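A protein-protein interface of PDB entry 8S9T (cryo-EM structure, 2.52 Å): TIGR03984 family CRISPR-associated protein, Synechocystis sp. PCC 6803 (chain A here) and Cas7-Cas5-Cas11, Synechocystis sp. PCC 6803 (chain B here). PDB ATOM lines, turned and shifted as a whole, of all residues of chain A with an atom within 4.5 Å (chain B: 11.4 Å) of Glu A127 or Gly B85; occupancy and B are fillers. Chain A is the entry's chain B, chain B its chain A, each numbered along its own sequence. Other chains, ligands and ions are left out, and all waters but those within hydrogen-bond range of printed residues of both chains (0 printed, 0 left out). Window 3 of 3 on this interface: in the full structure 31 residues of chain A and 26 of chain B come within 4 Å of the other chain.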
ATOM      1  N   GLY A 126     -31.716  24.014 -24.657  1.00  0.00           N
ATOM      2  CA  GLY A 126     -30.539  24.697 -24.166  1.00  0.00           C
ATOM      3  C   GLY A 126     -30.330  26.096 -24.720  1.00  0.00           C
ATOM      4  O   GLY A 126     -30.872  26.486 -25.753  1.00  0.00           O
ATOM      5  N   GLU A 127     -29.523  26.855 -23.989  1.00  0.00           N
ATOM      6  CA  GLU A 127     -28.903  28.144 -24.249  1.00  0.00           C
ATOM      7  C   GLU A 127     -27.483  27.947 -24.752  1.00  0.00           C
ATOM      8  O   GLU A 127     -26.853  26.931 -24.455  1.00  0.00           O
ATOM      9  CB  GLU A 127     -28.894  28.981 -22.971  1.00  0.00           C
ATOM     10  CG  GLU A 127     -30.276  29.327 -22.498  1.00  0.00           C
ATOM     11  CD  GLU A 127     -30.284  30.018 -21.163  1.00  0.00           C
ATOM     12  OE1 GLU A 127     -29.626  31.064 -21.023  1.00  0.00           O
ATOM     13  OE2 GLU A 127     -30.968  29.520 -20.249  1.00  0.00           O
ATOM     14  N   PRO A 128     -26.929  28.911 -25.492  1.00  0.00           N
ATOM     15  CA  PRO A 128     -25.558  28.762 -26.002  1.00  0.00           C
ATOM     16  C   PRO A 128     -24.550  28.560 -24.882  1.00  0.00           C
ATOM     17  O   PRO A 128     -24.525  29.309 -23.906  1.00  0.00           O
ATOM     18  CB  PRO A 128     -25.317  30.080 -26.739  1.00  0.00           C
ATOM     19  CG  PRO A 128     -26.632  30.546 -27.093  1.00  0.00           C
ATOM     20  CD  PRO A 128     -27.527  30.165 -25.970  1.00  0.00           C
ATOM     21  N   ALA A 129     -23.723  27.529 -25.028  1.00  0.00           N
ATOM     22  CA  ALA A 129     -22.722  27.239 -24.017  1.00  0.00           C
ATOM     23  C   ALA A 129     -21.643  28.313 -24.009  1.00  0.00           C
ATOM     24  O   ALA A 129     -21.458  29.062 -24.967  1.00  0.00           O
ATOM     25  CB  ALA A 129     -22.094  25.869 -24.246  1.00  0.00           C
ATOM     26  N   ARG A 140     -22.475  24.502 -29.068  1.00  0.00           N
ATOM     27  CA  ARG A 140     -22.977  23.770 -27.924  1.00  0.00           C
ATOM     28  C   ARG A 140     -24.070  24.584 -27.259  1.00  0.00           C
ATOM     29  O   ARG A 140     -23.837  25.716 -26.830  1.00  0.00           O
ATOM     30  CB  ARG A 140     -21.843  23.445 -26.963  1.00  0.00           C
ATOM     31  CG  ARG A 140     -22.258  22.660 -25.762  1.00  0.00           C
ATOM     32  CD  ARG A 140     -21.048  22.208 -25.011  1.00  0.00           C
ATOM     33  NE  ARG A 140     -20.319  21.198 -25.764  1.00  0.00           N
ATOM     34  CZ  ARG A 140     -19.049  20.892 -25.556  1.00  0.00           C
ATOM     35  NH1 ARG A 140     -18.382  21.486 -24.584  1.00  0.00           N
ATOM     36  NH2 ARG A 140     -18.460  19.961 -26.285  1.00  0.00           N
ATOM     37  N   LEU A 141     -25.268  24.023 -27.217  1.00  0.00           N
ATOM     38  CA  LEU A 141     -26.293  24.469 -26.296  1.00  0.00           C
ATOM     39  C   LEU A 141     -26.132  23.684 -25.014  1.00  0.00           C
ATOM     40  O   LEU A 141     -25.629  22.562 -25.025  1.00  0.00           O
ATOM     41  CB  LEU A 141     -27.681  24.253 -26.895  1.00  0.00           C
ATOM     42  CG  LEU A 141     -27.912  24.941 -28.239  1.00  0.00           C
ATOM     43  CD1 LEU A 141     -29.264  24.594 -28.793  1.00  0.00           C
ATOM     44  CD2 LEU A 141     -27.777  26.431 -28.098  1.00  0.00           C
ATOM     45  N   ALA A 142     -26.584  24.258 -23.910  1.00  0.00           N
ATOM     46  CA  ALA A 142     -26.675  23.464 -22.703  1.00  0.00           C
ATOM     47  C   ALA A 142     -27.821  23.956 -21.846  1.00  0.00           C
ATOM     48  O   ALA A 142     -28.167  25.136 -21.847  1.00  0.00           O
ATOM     49  CB  ALA A 142     -25.372  23.489 -21.913  1.00  0.00           C
ATOM     50  N   GLU A 143     -28.369  23.030 -21.078  1.00  0.00           N
ATOM     51  CA  GLU A 143     -29.438  23.274 -20.135  1.00  0.00           C
ATOM     52  C   GLU A 143     -29.187  22.325 -18.985  1.00  0.00           C
ATOM     53  O   GLU A 143     -28.732  21.203 -19.207  1.00  0.00           O
ATOM     54  CB  GLU A 143     -30.804  22.991 -20.760  1.00  0.00           C
ATOM     55  CG  GLU A 143     -31.962  23.466 -19.938  1.00  0.00           C
ATOM     56  CD  GLU A 143     -33.267  23.453 -20.691  1.00  0.00           C
ATOM     57  OE1 GLU A 143     -33.318  23.975 -21.824  1.00  0.00           O
ATOM     58  OE2 GLU A 143     -34.259  22.967 -20.115  1.00  0.00           O
ATOM     59  N   ALA A 144     -29.438  22.778 -17.760  1.00  0.00           N
ATOM     60  CA  ALA A 144     -29.165  21.918 -16.619  1.00  0.00           C
ATOM     61  C   ALA A 144     -29.955  20.630 -16.719  1.00  0.00           C
ATOM     62  O   ALA A 144     -29.519  19.586 -16.231  1.00  0.00           O
ATOM     63  CB  ALA A 144     -29.493  22.640 -15.321  1.00  0.00           C
ATOM     64  N   LYS A 160     -27.734  34.563 -25.285  1.00  0.00           N
ATOM     65  CA  LYS A 160     -29.179  34.736 -25.409  1.00  0.00           C
ATOM     66  C   LYS A 160     -29.716  34.532 -26.818  1.00  0.00           C
ATOM     67  O   LYS A 160     -30.872  34.879 -27.080  1.00  0.00           O
ATOM     68  CB  LYS A 160     -29.623  36.112 -24.899  1.00  0.00           C
ATOM     69  CG  LYS A 160     -29.189  36.395 -23.475  1.00  0.00           C
ATOM     70  CD  LYS A 160     -29.817  35.390 -22.525  1.00  0.00           C
ATOM     71  CE  LYS A 160     -29.391  35.617 -21.088  1.00  0.00           C
ATOM     72  NZ  LYS A 160     -30.040  34.646 -20.166  1.00  0.00           N
ATOM     73  N   ARG A 162     -31.305  31.713 -29.208  1.00  0.00           N
ATOM     74  CA  ARG A 162     -31.964  30.423 -29.096  1.00  0.00           C
ATOM     75  C   ARG A 162     -32.044  29.803 -30.475  1.00  0.00           C
ATOM     76  O   ARG A 162     -32.213  30.504 -31.472  1.00  0.00           O
ATOM     77  CB  ARG A 162     -33.360  30.537 -28.489  1.00  0.00           C
ATOM     78  CG  ARG A 162     -33.394  30.679 -26.989  1.00  0.00           C
ATOM     79  CD  ARG A 162     -32.826  29.453 -26.318  1.00  0.00           C
ATOM     80  NE  ARG A 162     -33.335  29.280 -24.964  1.00  0.00           N
ATOM     81  CZ  ARG A 162     -33.906  28.169 -24.511  1.00  0.00           C
ATOM     82  NH1 ARG A 162     -33.975  27.089 -25.266  1.00  0.00           N
ATOM     83  NH2 ARG A 162     -34.343  28.116 -23.270  1.00  0.00           N
ATOM     84  N   GLN B  79     -29.716  19.535  -8.705  1.00  0.00           N
ATOM     85  CA  GLN B  79     -31.068  20.080  -8.737  1.00  0.00           C
ATOM     86  C   GLN B  79     -31.311  20.901  -9.993  1.00  0.00           C
ATOM     87  O   GLN B  79     -31.445  22.122  -9.917  1.00  0.00           O
ATOM     88  CB  GLN B  79     -31.336  20.925  -7.506  1.00  0.00           C
ATOM     89  CG  GLN B  79     -31.261  20.155  -6.256  1.00  0.00           C
ATOM     90  CD  GLN B  79     -31.735  20.947  -5.104  1.00  0.00           C
ATOM     91  OE1 GLN B  79     -32.869  20.813  -4.674  1.00  0.00           O
ATOM     92  NE2 GLN B  79     -30.866  21.767  -4.566  1.00  0.00           N
ATOM     93  N   PRO B  80     -31.401  20.256 -11.155  1.00  0.00           N
ATOM     94  CA  PRO B  80     -31.409  20.997 -12.424  1.00  0.00           C
ATOM     95  C   PRO B  80     -32.535  21.999 -12.587  1.00  0.00           C
ATOM     96  O   PRO B  80     -32.380  22.958 -13.343  1.00  0.00           O
ATOM     97  CB  PRO B  80     -31.529  19.874 -13.458  1.00  0.00           C
ATOM     98  CG  PRO B  80     -32.109  18.754 -12.708  1.00  0.00           C
ATOM     99  CD  PRO B  80     -31.532  18.812 -11.376  1.00  0.00           C
ATOM    100  N   ALA B  81     -33.660  21.819 -11.903  1.00  0.00           N
ATOM    101  CA  ALA B  81     -34.750  22.778 -12.016  1.00  0.00           C
ATOM    102  C   ALA B  81     -34.383  24.140 -11.445  1.00  0.00           C
ATOM    103  O   ALA B  81     -34.959  25.152 -11.850  1.00  0.00           O
ATOM    104  CB  ALA B  81     -35.992  22.225 -11.331  1.00  0.00           C
ATOM    105  N   LEU B  82     -33.443  24.190 -10.514  1.00  0.00           N
ATOM    106  CA  LEU B  82     -32.997  25.453  -9.951  1.00  0.00           C
ATOM    107  C   LEU B  82     -31.850  26.078 -10.725  1.00  0.00           C
ATOM    108  O   LEU B  82     -31.720  27.304 -10.736  1.00  0.00           O
ATOM    109  CB  LEU B  82     -32.576  25.264  -8.495  1.00  0.00           C
ATOM    110  CG  LEU B  82     -33.590  24.574  -7.596  1.00  0.00           C
ATOM    111  CD1 LEU B  82     -33.074  24.598  -6.188  1.00  0.00           C
ATOM    112  CD2 LEU B  82     -34.947  25.246  -7.703  1.00  0.00           C
ATOM    113  N   ALA B  83     -31.003  25.270 -11.349  1.00  0.00           N
ATOM    114  CA  ALA B  83     -29.913  25.805 -12.151  1.00  0.00           C
ATOM    115  C   ALA B  83     -30.430  26.456 -13.427  1.00  0.00           C
ATOM    116  O   ALA B  83     -31.376  25.976 -14.059  1.00  0.00           O
ATOM    117  CB  ALA B  83     -28.924  24.698 -12.492  1.00  0.00           C
ATOM    118  N   GLN B  84     -29.782  27.545 -13.819  1.00  0.00           N
ATOM    119  CA  GLN B  84     -30.156  28.272 -15.018  1.00  0.00           C
ATOM    120  C   GLN B  84     -28.899  28.682 -15.764  1.00  0.00           C
ATOM    121  O   GLN B  84     -27.808  28.748 -15.200  1.00  0.00           O
ATOM    122  CB  GLN B  84     -31.027  29.481 -14.695  1.00  0.00           C
ATOM    123  CG  GLN B  84     -30.343  30.538 -13.876  1.00  0.00           C
ATOM    124  CD  GLN B  84     -31.222  31.747 -13.682  1.00  0.00           C
ATOM    125  OE1 GLN B  84     -30.974  32.810 -14.251  1.00  0.00           O
ATOM    126  NE2 GLN B  84     -32.272  31.589 -12.888  1.00  0.00           N
ATOM    127  N   GLY B  85     -29.071  28.949 -17.050  1.00  0.00           N
ATOM    128  CA  GLY B  85     -27.956  29.076 -17.950  1.00  0.00           C
ATOM    129  C   GLY B  85     -27.456  27.738 -18.459  1.00  0.00           C
ATOM    130  O   GLY B  85     -28.032  26.674 -18.220  1.00  0.00           O
ATOM    131  N   ALA B  86     -26.344  27.812 -19.187  1.00  0.00           N
ATOM    132  CA  ALA B  86     -25.844  26.703 -19.993  1.00  0.00           C
ATOM    133  C   ALA B  86     -25.034  25.713 -19.154  1.00  0.00           C
ATOM    134  O   ALA B  86     -23.821  25.569 -19.302  1.00  0.00           O
ATOM    135  CB  ALA B  86     -25.022  27.240 -21.152  1.00  0.00           C
ATOM    136  N   ILE B  87     -25.723  25.030 -18.243  1.00  0.00           N
ATOM    137  CA  ILE B  87     -25.077  23.965 -17.476  1.00  0.00           C
ATOM    138  C   ILE B  87     -24.780  22.802 -18.420  1.00  0.00           C
ATOM    139  O   ILE B  87     -25.699  22.135 -18.900  1.00  0.00           O
ATOM    140  CB  ILE B  87     -25.924  23.513 -16.280  1.00  0.00           C
ATOM    141  CG1 ILE B  87     -25.843  24.509 -15.119  1.00  0.00           C
ATOM    142  CG2 ILE B  87     -25.459  22.172 -15.785  1.00  0.00           C
ATOM    143  CD1 ILE B  87     -26.471  25.828 -15.348  1.00  0.00           C
ATOM    144  N   GLU B  88     -23.498  22.580 -18.713  1.00  0.00           N
ATOM    145  CA  GLU B  88     -23.039  21.540 -19.628  1.00  0.00           C
ATOM    146  C   GLU B  88     -23.041  20.111 -19.096  1.00  0.00           C
ATOM    147  O   GLU B  88     -23.318  19.193 -19.874  1.00  0.00           O
ATOM    148  CB  GLU B  88     -21.636  21.872 -20.151  1.00  0.00           C
ATOM    149  CG  GLU B  88     -21.532  23.189 -20.913  1.00  0.00           C
ATOM    150  CD  GLU B  88     -21.228  24.381 -20.035  1.00  0.00           C
ATOM    151  OE1 GLU B  88     -20.862  25.440 -20.590  1.00  0.00           O
ATOM    152  OE2 GLU B  88     -21.347  24.262 -18.795  1.00  0.00           O
ATOM    153  N   PRO B  89     -22.710  19.844 -17.831  1.00  0.00           N
ATOM    154  CA  PRO B  89     -22.742  18.455 -17.365  1.00  0.00           C
ATOM    155  C   PRO B  89     -24.163  17.934 -17.224  1.00  0.00           C
ATOM    156  O   PRO B  89     -25.063  18.644 -16.770  1.00  0.00           O
ATOM    157  CB  PRO B  89     -22.026  18.519 -16.017  1.00  0.00           C
ATOM    158  CG  PRO B  89     -22.221  19.886 -15.565  1.00  0.00           C
ATOM    159  CD  PRO B  89     -22.186  20.735 -16.784  1.00  0.00           C
ATOM    160  N   GLU B  90     -24.352  16.674 -17.600  1.00  0.00           N
ATOM    161  CA  GLU B  90     -25.625  16.009 -17.368  1.00  0.00           C
ATOM    162  C   GLU B  90     -25.950  16.012 -15.881  1.00  0.00           C
ATOM    163  O   GLU B  90     -25.044  15.913 -15.048  1.00  0.00           O
ATOM    164  CB  GLU B  90     -25.595  14.572 -17.878  1.00  0.00           C
ATOM    165  CG  GLU B  90     -25.575  14.447 -19.374  1.00  0.00           C
ATOM    166  CD  GLU B  90     -25.370  13.023 -19.839  1.00  0.00           C
ATOM    167  OE1 GLU B  90     -25.935  12.103 -19.213  1.00  0.00           O
ATOM    168  OE2 GLU B  90     -24.641  12.823 -20.833  1.00  0.00           O
ATOM    169  N   PRO B  91     -27.222  16.141 -15.512  1.00  0.00           N
ATOM    170  CA  PRO B  91     -27.577  16.129 -14.092  1.00  0.00           C
ATOM    171  C   PRO B  91     -27.286  14.777 -13.454  1.00  0.00           C
ATOM    172  O   PRO B  91     -27.723  13.736 -13.939  1.00  0.00           O
ATOM    173  CB  PRO B  91     -29.072  16.461 -14.107  1.00  0.00           C
ATOM    174  CG  PRO B  91     -29.526  16.064 -15.425  1.00  0.00           C
ATOM    175  CD  PRO B  91     -28.406  16.277 -16.371  1.00  0.00           C
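O of Ile B87 sits close to O of Glu A143 (3.2 Å).
Among the printed residues, merely in contact across the chains: Glu A127 with Gly B85 (3.8 Å), Glu A127 with Ala B86 (3.8 Å), Pro A128 with Ala B86 (3.5 Å), Ala A129 with Ala B86 (3.7 Å), Ala A129 with Glu B88 (3.9 Å), Ala A142 with Gly B85 (3.9 Å), Ala A142 with Ala B86 (3.4 Å), Ala A142 with Ile B87 (3.3 Å), Ala A142 with Glu B88 (3.8 Å), Ala A144 with Pro B80 (3.4 Å), Ala A144 with Ala B83 (3.5 Å), Ala A144 with Ile B87 (3.6 Å) and Ala A144 with Pro B91 (3.5 Å).
Of chain A, only Glu A127 (3.8 Å) and Ala A142 (3.9 Å) come within 4 Å of Gly B85.
No residue of chain B comes within 4 Å of Gly A126.
Of chain B, only Ala B86 (3.5 Å) comes within 4 Å of Pro A128.
Of chain B, only Ala B86 and Glu B88 come within 4 Å of Ala A129.
Lys A160 touches none of the printed residues of chain B.
Printed residues of chain A within 4 Å of Ala B83: Ala A144.
Of the printed residues of chain B, Ala A144 touches Pro B80, Ala B83, Ile B87 and Pro B91.
Printed residues of chain A within 4 Å of Ala B86: Glu A127 (3.8 Å), Pro A128 (3.5 Å), Ala A129 (3.7 Å) and Ala A142 (3.4 Å).
Pro B89 touches none of the printed residues of chain A.
Arg A162 touches none of the printed residues of chain B.
The nearest residue of chain B that does not touch Glu A127 is Gln B84 (5.0 Å).
The nearest printed residue of chain A that does not touch Gly B85 is Glu A143 (4.1 Å).
The backbone NH (N) of Gly A126 sits at hydrogen-bond distance from the side-chain carboxylate (OE1) of Glu A143, 3.3 Å away.
The backbone carbonyl oxygen (O) of Glu A127 sits at hydrogen-bond distance from the backbone NH (N) of Ala A142, 2.7 Å away.
The backbone carbonyl oxygen of Arg A140 lies within hydrogen-bond range of the backbone NH of Ala A129 (2.6 Å).
The side-chain carboxylate of Glu A127 lies within salt-bridge range of the side-chain amino group of Lys A160, 3.7 Å away.
Hydrophobic or aromatic side chains of chain A that line the printed part of chain B: Ala A129, Ala A142 and Ala A144.
Of the 13 printed residues of chain B, 7 touch a printed residue of chain A.
Hydrophobic or aromatic side chains of chain B within 4 Å of the printed part of chain A: Pro B80, Ala B83, Ala B86, Ile B87 and Pro B91.
Among the printed residues, no Asp or Glu carboxylate lies within 4 Å of a Lys or Arg side-chain nitrogen of the other chain.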
